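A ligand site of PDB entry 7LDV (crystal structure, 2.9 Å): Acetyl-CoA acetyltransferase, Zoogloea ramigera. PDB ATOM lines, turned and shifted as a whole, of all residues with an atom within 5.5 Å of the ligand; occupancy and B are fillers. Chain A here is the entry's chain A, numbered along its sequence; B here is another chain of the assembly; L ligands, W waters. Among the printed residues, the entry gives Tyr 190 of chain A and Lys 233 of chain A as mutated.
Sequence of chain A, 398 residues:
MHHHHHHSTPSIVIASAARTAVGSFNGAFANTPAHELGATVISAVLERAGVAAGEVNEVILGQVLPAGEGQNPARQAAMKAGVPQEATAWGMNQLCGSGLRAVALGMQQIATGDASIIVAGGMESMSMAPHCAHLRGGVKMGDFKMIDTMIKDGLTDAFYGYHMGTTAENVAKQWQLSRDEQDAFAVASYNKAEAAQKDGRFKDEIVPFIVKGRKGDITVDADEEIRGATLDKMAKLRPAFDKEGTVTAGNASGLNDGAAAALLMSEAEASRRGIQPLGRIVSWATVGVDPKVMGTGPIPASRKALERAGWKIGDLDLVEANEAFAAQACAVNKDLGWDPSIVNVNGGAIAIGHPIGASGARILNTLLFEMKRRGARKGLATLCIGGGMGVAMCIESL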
ATOM      1  N   SCY A  96      37.663  15.031  20.779  1.00  0.00           N
ATOM      2  CA  SCY A  96      37.485  15.140  22.221  1.00  0.00           C
ATOM      3  CB  SCY A  96      37.575  13.777  22.886  1.00  0.00           C
ATOM      4  SG  SCY A  96      36.263  12.689  22.358  1.00  0.00           S
ATOM      5  CD  SCY A  96      36.792  11.943  20.912  1.00  0.00           C
ATOM      6  OCD SCY A  96      37.946  11.893  20.455  1.00  0.00           O
ATOM      7  CE  SCY A  96      35.630  11.325  20.195  1.00  0.00           C
ATOM      8  C   SCY A  96      38.498  16.097  22.953  1.00  0.00           C
ATOM      9  O   SCY A  96      38.231  16.483  24.127  1.00  0.00           O
ATOM     10  N   LEU A 155      31.775   9.655  16.655  1.00  0.00           N
ATOM     11  CA  LEU A 155      31.982   8.480  17.480  1.00  0.00           C
ATOM     12  C   LEU A 155      32.463   7.253  16.722  1.00  0.00           C
ATOM     13  O   LEU A 155      32.656   6.200  17.337  1.00  0.00           O
ATOM     14  CB  LEU A 155      30.675   8.135  18.215  1.00  0.00           C
ATOM     15  CG  LEU A 155      30.061   9.260  19.046  1.00  0.00           C
ATOM     16  CD1 LEU A 155      28.781   8.791  19.721  1.00  0.00           C
ATOM     17  CD2 LEU A 155      31.054   9.777  20.077  1.00  0.00           C
ATOM     18  N   HIS A 163      32.804   1.756  16.417  1.00  0.00           N
ATOM     19  CA  HIS A 163      32.569   2.808  17.398  1.00  0.00           C
ATOM     20  C   HIS A 163      33.792   2.993  18.292  1.00  0.00           C
ATOM     21  O   HIS A 163      34.657   2.120  18.395  1.00  0.00           O
ATOM     22  CB  HIS A 163      31.329   2.469  18.228  1.00  0.00           C
ATOM     23  CG  HIS A 163      30.753   3.638  18.967  1.00  0.00           C
ATOM     24  ND1 HIS A 163      31.220   4.055  20.192  1.00  0.00           N
ATOM     25  CD2 HIS A 163      29.723   4.457  18.663  1.00  0.00           C
ATOM     26  CE1 HIS A 163      30.508   5.090  20.608  1.00  0.00           C
ATOM     27  NE2 HIS A 163      29.591   5.355  19.694  1.00  0.00           N
ATOM     28  N   MET A 164      33.843   4.154  18.953  1.00  0.00           N
ATOM     29  CA  MET A 164      34.906   4.409  19.926  1.00  0.00           C
ATOM     30  C   MET A 164      34.858   3.411  21.079  1.00  0.00           C
ATOM     31  O   MET A 164      35.888   3.145  21.710  1.00  0.00           O
ATOM     32  CB  MET A 164      34.789   5.836  20.470  1.00  0.00           C
ATOM     33  CG  MET A 164      35.110   6.932  19.461  1.00  0.00           C
ATOM     34  SD  MET A 164      36.870   7.065  19.097  1.00  0.00           S
ATOM     35  CE  MET A 164      37.023   6.085  17.608  1.00  0.00           C
ATOM     36  N   GLY A 165      33.687   2.841  21.367  1.00  0.00           N
ATOM     37  CA  GLY A 165      33.596   1.836  22.401  1.00  0.00           C
ATOM     38  C   GLY A 165      34.346   0.566  22.063  1.00  0.00           C
ATOM     39  O   GLY A 165      34.828  -0.125  22.962  1.00  0.00           O
ATOM     40  N   TYR A 190      30.911   7.593  39.990  1.00  0.00           N
ATOM     41  CA  TYR A 190      29.570   8.081  40.315  1.00  0.00           C
ATOM     42  C   TYR A 190      29.498   8.574  41.759  1.00  0.00           C
ATOM     43  O   TYR A 190      28.854   9.603  42.038  1.00  0.00           O
ATOM     44  CB  TYR A 190      28.538   6.983  40.075  1.00  0.00           C
ATOM     45  CG  TYR A 190      27.941   6.982  38.688  1.00  0.00           C
ATOM     46  CD1 TYR A 190      26.935   7.878  38.344  1.00  0.00           C
ATOM     47  CD2 TYR A 190      28.375   6.086  37.727  1.00  0.00           C
ATOM     48  CE1 TYR A 190      26.382   7.884  37.077  1.00  0.00           C
ATOM     49  CE2 TYR A 190      27.827   6.088  36.451  1.00  0.00           C
ATOM     50  CZ  TYR A 190      26.837   6.981  36.134  1.00  0.00           C
ATOM     51  OH  TYR A 190      26.294   6.983  34.875  1.00  0.00           O
ATOM     52  N   ARG A 227      23.763  10.557  38.879  1.00  0.00           N
ATOM     53  CA  ARG A 227      22.729   9.771  39.540  1.00  0.00           C
ATOM     54  C   ARG A 227      23.367   8.917  40.636  1.00  0.00           C
ATOM     55  O   ARG A 227      24.534   9.107  41.010  1.00  0.00           O
ATOM     56  CB  ARG A 227      21.985   8.907  38.524  1.00  0.00           C
ATOM     57  CG  ARG A 227      22.881   7.984  37.718  1.00  0.00           C
ATOM     58  CD  ARG A 227      22.085   6.973  36.896  1.00  0.00           C
ATOM     59  NE  ARG A 227      21.660   5.828  37.691  1.00  0.00           N
ATOM     60  CZ  ARG A 227      20.897   4.836  37.240  1.00  0.00           C
ATOM     61  NH1 ARG A 227      20.460   4.855  35.990  1.00  0.00           N
ATOM     62  NH2 ARG A 227      20.570   3.826  38.038  1.00  0.00           N
ATOM     63  N   ALA A 229      24.559   5.204  41.633  1.00  0.00           N
ATOM     64  CA  ALA A 229      24.954   3.951  41.006  1.00  0.00           C
ATOM     65  C   ALA A 229      25.241   2.899  42.069  1.00  0.00           C
ATOM     66  O   ALA A 229      25.925   3.187  43.061  1.00  0.00           O
ATOM     67  CB  ALA A 229      26.174   4.142  40.112  1.00  0.00           C
ATOM     68  N   LYS A 233      23.225  -3.416  40.192  1.00  0.00           N
ATOM     69  CA  LYS A 233      22.481  -3.013  38.999  1.00  0.00           C
ATOM     70  C   LYS A 233      23.408  -2.698  37.825  1.00  0.00           C
ATOM     71  O   LYS A 233      23.030  -2.898  36.670  1.00  0.00           O
ATOM     72  CB  LYS A 233      21.580  -1.822  39.306  1.00  0.00           C
ATOM     73  CG  LYS A 233      20.410  -2.150  40.217  1.00  0.00           C
ATOM     74  CD  LYS A 233      19.406  -1.013  40.285  1.00  0.00           C
ATOM     75  CE  LYS A 233      20.016   0.238  40.887  1.00  0.00           C
ATOM     76  NZ  LYS A 233      19.009   1.332  41.017  1.00  0.00           N
ATOM     77  N   MET A 234      24.621  -2.215  38.106  1.00  0.00           N
ATOM     78  CA  MET A 234      25.571  -1.960  37.034  1.00  0.00           C
ATOM     79  C   MET A 234      26.105  -3.244  36.425  1.00  0.00           C
ATOM     80  O   MET A 234      26.377  -3.304  35.219  1.00  0.00           O
ATOM     81  CB  MET A 234      26.722  -1.080  37.544  1.00  0.00           C
ATOM     82  CG  MET A 234      27.627  -0.560  36.439  1.00  0.00           C
ATOM     83  SD  MET A 234      28.373   1.022  36.853  1.00  0.00           S
ATOM     84  CE  MET A 234      26.910   1.977  37.260  1.00  0.00           C
ATOM     85  N   LEU A 237      23.937  -4.921  33.508  1.00  0.00           N
ATOM     86  CA  LEU A 237      23.801  -4.311  32.196  1.00  0.00           C
ATOM     87  C   LEU A 237      24.492  -5.162  31.131  1.00  0.00           C
ATOM     88  O   LEU A 237      25.473  -5.848  31.393  1.00  0.00           O
ATOM     89  CB  LEU A 237      24.382  -2.896  32.194  1.00  0.00           C
ATOM     90  CG  LEU A 237      23.811  -1.914  33.213  1.00  0.00           C
ATOM     91  CD1 LEU A 237      24.531  -0.582  33.139  1.00  0.00           C
ATOM     92  CD2 LEU A 237      22.315  -1.731  32.993  1.00  0.00           C
ATOM     93  N   ALA A 240      27.331  -2.925  25.286  1.00  0.00           N
ATOM     94  CA  ALA A 240      26.696  -2.039  24.321  1.00  0.00           C
ATOM     95  C   ALA A 240      27.312  -2.101  22.937  1.00  0.00           C
ATOM     96  O   ALA A 240      26.679  -1.632  21.980  1.00  0.00           O
ATOM     97  CB  ALA A 240      26.748  -0.596  24.838  1.00  0.00           C
ATOM     98  N   PHE A 241      28.518  -2.652  22.794  1.00  0.00           N
ATOM     99  CA  PHE A 241      29.202  -2.667  21.509  1.00  0.00           C
ATOM    100  C   PHE A 241      29.483  -4.100  21.065  1.00  0.00           C
ATOM    101  O   PHE A 241      28.805  -4.593  20.166  1.00  0.00           O
ATOM    102  CB  PHE A 241      30.484  -1.845  21.580  1.00  0.00           C
ATOM    103  CG  PHE A 241      30.283  -0.454  22.115  1.00  0.00           C
ATOM    104  CD1 PHE A 241      29.776   0.553  21.301  1.00  0.00           C
ATOM    105  CD2 PHE A 241      30.605  -0.146  23.423  1.00  0.00           C
ATOM    106  CE1 PHE A 241      29.577   1.828  21.796  1.00  0.00           C
ATOM    107  CE2 PHE A 241      30.414   1.133  23.921  1.00  0.00           C
ATOM    108  CZ  PHE A 241      29.908   2.116  23.108  1.00  0.00           C
ATOM    109  N   THR A 248      29.910  -1.511  28.868  1.00  0.00           N
ATOM    110  CA  THR A 248      28.459  -1.368  28.913  1.00  0.00           C
ATOM    111  C   THR A 248      28.093   0.111  29.007  1.00  0.00           C
ATOM    112  O   THR A 248      28.959   0.989  29.073  1.00  0.00           O
ATOM    113  CB  THR A 248      27.875  -2.146  30.099  1.00  0.00           C
ATOM    114  OG1 THR A 248      28.337  -1.578  31.329  1.00  0.00           O
ATOM    115  CG2 THR A 248      28.280  -3.608  30.035  1.00  0.00           C
ATOM    116  N   ALA A 249      26.790   0.381  29.028  1.00  0.00           N
ATOM    117  CA  ALA A 249      26.313   1.754  29.146  1.00  0.00           C
ATOM    118  C   ALA A 249      26.656   2.370  30.496  1.00  0.00           C
ATOM    119  O   ALA A 249      26.663   3.593  30.626  1.00  0.00           O
ATOM    120  CB  ALA A 249      24.803   1.818  28.903  1.00  0.00           C
ATOM    121  N   GLY A 250      26.922   1.541  31.513  1.00  0.00           N
ATOM    122  CA  GLY A 250      27.242   2.034  32.836  1.00  0.00           C
ATOM    123  C   GLY A 250      28.670   2.491  32.998  1.00  0.00           C
ATOM    124  O   GLY A 250      28.922   3.576  33.544  1.00  0.00           O
ATOM    125  N   ALA A 252      30.715   3.391  30.693  1.00  0.00           N
ATOM    126  CA  ALA A 252      31.113   4.257  29.598  1.00  0.00           C
ATOM    127  C   ALA A 252      30.423   5.600  29.723  1.00  0.00           C
ATOM    128  O   ALA A 252      29.270   5.687  30.160  1.00  0.00           O
ATOM    129  CB  ALA A 252      30.783   3.616  28.245  1.00  0.00           C
ATOM    130  N   SER A 253      31.134   6.657  29.331  1.00  0.00           N
ATOM    131  CA  SER A 253      30.533   7.986  29.337  1.00  0.00           C
ATOM    132  C   SER A 253      29.395   8.052  28.333  1.00  0.00           C
ATOM    133  O   SER A 253      29.318   7.282  27.369  1.00  0.00           O
ATOM    134  CB  SER A 253      31.587   9.049  29.027  1.00  0.00           C
ATOM    135  OG  SER A 253      32.152   8.846  27.739  1.00  0.00           O
ATOM    136  N   GLY A 254      28.478   9.001  28.565  1.00  0.00           N
ATOM    137  CA  GLY A 254      27.305   9.145  27.733  1.00  0.00           C
ATOM    138  C   GLY A 254      27.420  10.301  26.750  1.00  0.00           C
ATOM    139  O   GLY A 254      28.442  10.968  26.627  1.00  0.00           O
ATOM    140  N   LEU A 255      26.319  10.517  26.033  1.00  0.00           N
ATOM    141  CA  LEU A 255      26.205  11.621  25.097  1.00  0.00           C
ATOM    142  C   LEU A 255      25.627  12.822  25.830  1.00  0.00           C
ATOM    143  O   LEU A 255      24.616  12.693  26.536  1.00  0.00           O
ATOM    144  CB  LEU A 255      25.328  11.231  23.912  1.00  0.00           C
ATOM    145  CG  LEU A 255      25.513   9.793  23.420  1.00  0.00           C
ATOM    146  CD1 LEU A 255      24.476   9.434  22.363  1.00  0.00           C
ATOM    147  CD2 LEU A 255      26.919   9.575  22.895  1.00  0.00           C
ATOM    148  N   MET A 294      43.028   4.290  20.884  1.00  0.00           N
ATOM    149  CA  MET A 294      43.067   5.735  21.071  1.00  0.00           C
ATOM    150  C   MET A 294      42.930   6.123  22.544  1.00  0.00           C
ATOM    151  O   MET A 294      43.282   7.250  22.907  1.00  0.00           O
ATOM    152  CB  MET A 294      41.972   6.410  20.247  1.00  0.00           C
ATOM    153  CG  MET A 294      40.549   6.071  20.674  1.00  0.00           C
ATOM    154  SD  MET A 294      39.908   7.180  21.948  1.00  0.00           S
ATOM    155  CE  MET A 294      38.382   6.351  22.380  1.00  0.00           C
ATOM    156  N   ALA A 324      36.656   8.818  29.344  1.00  0.00           N
ATOM    157  CA  ALA A 324      35.831   8.434  28.204  1.00  0.00           C
ATOM    158  C   ALA A 324      35.225   7.048  28.413  1.00  0.00           C
ATOM    159  O   ALA A 324      34.040   6.830  28.148  1.00  0.00           O
ATOM    160  CB  ALA A 324      36.665   8.468  26.926  1.00  0.00           C
ATOM    161  N   PHE A 325      36.027   6.100  28.887  1.00  0.00           N
ATOM    162  CA  PHE A 325      35.567   4.761  29.208  1.00  0.00           C
ATOM    163  C   PHE A 325      36.290   4.282  30.457  1.00  0.00           C
ATOM    164  O   PHE A 325      37.400   4.737  30.764  1.00  0.00           O
ATOM    165  CB  PHE A 325      35.813   3.784  28.046  1.00  0.00           C
ATOM    166  CG  PHE A 325      35.113   4.157  26.780  1.00  0.00           C
ATOM    167  CD1 PHE A 325      33.823   3.731  26.533  1.00  0.00           C
ATOM    168  CD2 PHE A 325      35.747   4.936  25.825  1.00  0.00           C
ATOM    169  CE1 PHE A 325      33.169   4.074  25.368  1.00  0.00           C
ATOM    170  CE2 PHE A 325      35.096   5.282  24.647  1.00  0.00           C
ATOM    171  CZ  PHE A 325      33.807   4.853  24.430  1.00  0.00           C
ATOM    172  N   HIS A 354      30.039  13.756  29.001  1.00  0.00           N
ATOM    173  CA  HIS A 354      31.119  13.874  28.014  1.00  0.00           C
ATOM    174  C   HIS A 354      30.626  14.633  26.790  1.00  0.00           C
ATOM    175  O   HIS A 354      30.326  14.044  25.747  1.00  0.00           O
ATOM    176  CB  HIS A 354      31.644  12.488  27.615  1.00  0.00           C
ATOM    177  CG  HIS A 354      32.939  12.526  26.871  1.00  0.00           C
ATOM    178  ND1 HIS A 354      33.692  13.674  26.736  1.00  0.00           N
ATOM    179  CD2 HIS A 354      33.622  11.552  26.216  1.00  0.00           C
ATOM    180  CE1 HIS A 354      34.769  13.406  26.030  1.00  0.00           C
ATOM    181  NE2 HIS A 354      34.752  12.125  25.699  1.00  0.00           N
ATOM    182  N   ILE A 356      31.630  16.310  23.667  1.00  0.00           N
ATOM    183  CA  ILE A 356      32.874  16.066  22.927  1.00  0.00           C
ATOM    184  C   ILE A 356      33.695  17.340  22.793  1.00  0.00           C
ATOM    185  O   ILE A 356      34.836  17.419  23.280  1.00  0.00           O
ATOM    186  CB  ILE A 356      32.553  15.450  21.552  1.00  0.00           C
ATOM    187  CG1 ILE A 356      31.486  14.367  21.679  1.00  0.00           C
ATOM    188  CG2 ILE A 356      33.828  14.935  20.892  1.00  0.00           C
ATOM    189  CD1 ILE A 356      31.976  13.147  22.442  1.00  0.00           C
ATOM    190  N   CYS A 384      41.814  11.793  25.954  1.00  0.00           N
ATOM    191  CA  CYS A 384      42.092  10.963  24.798  1.00  0.00           C
ATOM    192  C   CYS A 384      41.275  11.464  23.607  1.00  0.00           C
ATOM    193  O   CYS A 384      40.167  11.990  23.775  1.00  0.00           O
ATOM    194  CB  CYS A 384      41.787   9.489  25.073  1.00  0.00           C
ATOM    195  SG  CYS A 384      40.041   9.117  25.341  1.00  0.00           S
ATOM    196  N   GLY A 386      39.850  10.702  19.561  1.00  0.00           N
ATOM    197  CA  GLY A 386      39.589   9.709  18.531  1.00  0.00           C
ATOM    198  C   GLY A 386      40.574   9.816  17.380  1.00  0.00           C
ATOM    199  O   GLY A 386      41.148  10.874  17.121  1.00  0.00           O
ATOM    200  N   MET B 141      18.722   7.849  17.865  1.00  0.00           N
ATOM    201  CA  MET B 141      20.131   7.540  17.686  1.00  0.00           C
ATOM    202  C   MET B 141      20.252   6.574  16.527  1.00  0.00           C
ATOM    203  O   MET B 141      19.362   5.746  16.310  1.00  0.00           O
ATOM    204  CB  MET B 141      20.733   6.909  18.951  1.00  0.00           C
ATOM    205  CG  MET B 141      22.251   6.853  18.956  1.00  0.00           C
ATOM    206  SD  MET B 141      22.983   6.030  20.404  1.00  0.00           S
ATOM    207  CE  MET B 141      21.572   5.073  20.973  1.00  0.00           C
HETATM  208  N1  LIG L   1      23.674   2.579  36.189  1.00  0.00           N
HETATM  209  C1  LIG L   1      22.776   1.613  36.045  1.00  0.00           C
HETATM  210  N2  LIG L   1      22.118   1.409  34.916  1.00  0.00           N
HETATM  211  C2  LIG L   1      22.342   2.189  33.859  1.00  0.00           C
HETATM  212  C3  LIG L   1      23.282   3.220  33.995  1.00  0.00           C
HETATM  213  C4  LIG L   1      23.944   3.393  35.183  1.00  0.00           C
HETATM  214  N3  LIG L   1      24.857   4.410  35.256  1.00  0.00           N
HETATM  215  N4  LIG L   1      23.362   3.896  32.832  1.00  0.00           N
HETATM  216  C5  LIG L   1      22.553   3.366  32.011  1.00  0.00           C
HETATM  217  N5  LIG L   1      21.901   2.318  32.572  1.00  0.00           N
HETATM  218  C6  LIG L   1      20.875   1.513  31.865  1.00  0.00           C
HETATM  219  C7  LIG L   1      19.633   2.364  31.547  1.00  0.00           C
HETATM  220  O1  LIG L   1      18.681   2.525  32.610  1.00  0.00           O
HETATM  221  C8  LIG L   1      18.996   1.551  30.376  1.00  0.00           C
HETATM  222  O2  LIG L   1      18.216   0.443  30.857  1.00  0.00           O
HETATM  223  P1  LIG L   1      16.712   0.587  30.320  1.00  0.00           P
HETATM  224  O3  LIG L   1      16.047  -0.735  30.480  1.00  0.00           O
HETATM  225  O4  LIG L   1      15.938   1.704  31.206  1.00  0.00           O
HETATM  226  O5  LIG L   1      16.712   1.009  28.753  1.00  0.00           O
HETATM  227  C9  LIG L   1      20.258   1.042  29.624  1.00  0.00           C
HETATM  228  O6  LIG L   1      21.344   1.084  30.533  1.00  0.00           O
HETATM  229  C10 LIG L   1      20.518   1.904  28.372  1.00  0.00           C
HETATM  230  O7  LIG L   1      21.386   3.006  28.632  1.00  0.00           O
HETATM  231  P2  LIG L   1      20.950   4.244  27.683  1.00  0.00           P
HETATM  232  O8  LIG L   1      20.729   5.416  28.566  1.00  0.00           O
HETATM  233  O9  LIG L   1      19.555   3.955  26.904  1.00  0.00           O
HETATM  234  O10 LIG L   1      22.138   4.648  26.662  1.00  0.00           O
HETATM  235  P3  LIG L   1      22.249   3.708  25.348  1.00  0.00           P
HETATM  236  O11 LIG L   1      22.105   2.298  25.736  1.00  0.00           O
HETATM  237  O12 LIG L   1      21.070   4.137  24.325  1.00  0.00           O
HETATM  238  O13 LIG L   1      23.682   3.959  24.618  1.00  0.00           O
HETATM  239  C11 LIG L   1      26.081   4.144  24.909  1.00  0.00           C
HETATM  240  C12 LIG L   1      24.725   3.958  25.602  1.00  0.00           C
HETATM  241  C13 LIG L   1      27.181   3.606  25.820  1.00  0.00           C
HETATM  242  C14 LIG L   1      26.073   3.331  23.617  1.00  0.00           C
HETATM  243  C15 LIG L   1      26.322   5.629  24.598  1.00  0.00           C
HETATM  244  O14 LIG L   1      26.185   6.375  25.803  1.00  0.00           O
HETATM  245  C16 LIG L   1      27.685   5.895  23.998  1.00  0.00           C
HETATM  246  O15 LIG L   1      27.850   5.799  22.807  1.00  0.00           O
HETATM  247  N6  LIG L   1      28.727   6.285  24.762  1.00  0.00           N
HETATM  248  C17 LIG L   1      30.029   6.530  24.133  1.00  0.00           C
HETATM  249  C18 LIG L   1      30.420   8.008  24.260  1.00  0.00           C
HETATM  250  C19 LIG L   1      31.720   8.272  23.552  1.00  0.00           C
HETATM  251  O16 LIG L   1      32.125   7.505  22.712  1.00  0.00           O
HETATM  252  N7  LIG L   1      32.450   9.362  23.873  1.00  0.00           N
HETATM  253  C20 LIG L   1      33.723   9.631  23.197  1.00  0.00           C
HETATM  254  C21 LIG L   1      34.817   8.752  23.803  1.00  0.00           C
HETATM  255  S1  LIG L   1      36.435   9.305  23.215  1.00  0.00           S
HETATM  256  O   HOH W   1      16.909   3.830  34.700  1.00  0.00           O
HETATM  257  O   HOH W   2      22.258   7.090  25.825  1.00  0.00           O
HETATM  258  O   HOH W   3      30.654  11.256  24.725  1.00  0.00           O
HETATM  259  O   HOH W   4      26.565   5.983  28.196  1.00  0.00           O
HETATM  260  O   HOH W   5      24.056   8.460  27.521  1.00  0.00           O
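Residues that only touch the ligand: Leu 155 (3.6 Å), His 163 (3.5 Å), Met 164 (3.9 Å), Arg 227 (3.7 Å), Met 234 (3.5 Å), Leu 237 (3.6 Å), Ala 249 (3.6 Å), Gly 254 (3.6 Å), Leu 255 (3.9 Å), Met 294 (3.6 Å), Ala 324 (3.6 Å), Phe 325 (3.6 Å), His 354 (3.4 Å), Ile 356 (3.998 Å) and Met 141 of chain B (3.5 Å).
18 residues have an atom within 4 Å of the ligand: SCY 96, Leu 155, His 163, Met 164, Tyr 190, Arg 227, Met 234, Leu 237, Ala 249, Ser 253, Gly 254, Leu 255, Met 294, Ala 324, Phe 325, His 354, Ile 356 and Met 141 of chain B.
Water W3 lies within hydrogen-bond range of a nitrogen (N7) of the ligand (2.7 Å), the backbone carbonyl oxygen of Gly 254 (2.9 Å) and the backbone carbonyl oxygen of His 354 (3.0 Å).
Water W5 lies within hydrogen-bond range of N of Leu 255 (3.4 Å) and O14 of the ligand (3.4 Å).
The backbone carbonyl oxygen (O) of Leu 155 lies within hydrogen-bond range of the backbone NH (N) of Met 164.
NE2 of His 354 lies within hydrogen-bond range of SG of SCY 96.
ND1 of His 163 lies within hydrogen-bond range of N of Gly 165.
O of Ala 324 lies within hydrogen-bond range of OG of Ser 253 (2.8 Å).
OCD of SCY 96 sits at hydrogen-bond distance from the backbone NH of Gly 386.
The backbone carbonyl oxygen (O) of Ser 253 lies within hydrogen-bond range of a nitrogen (N6) of the ligand (2.9 Å).
A nitrogen (N3) of the ligand sits at hydrogen-bond distance from the side-chain hydroxyl of Tyr 190 (3.0 Å).
SG of SCY 96 sits close to S1 of the ligand.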
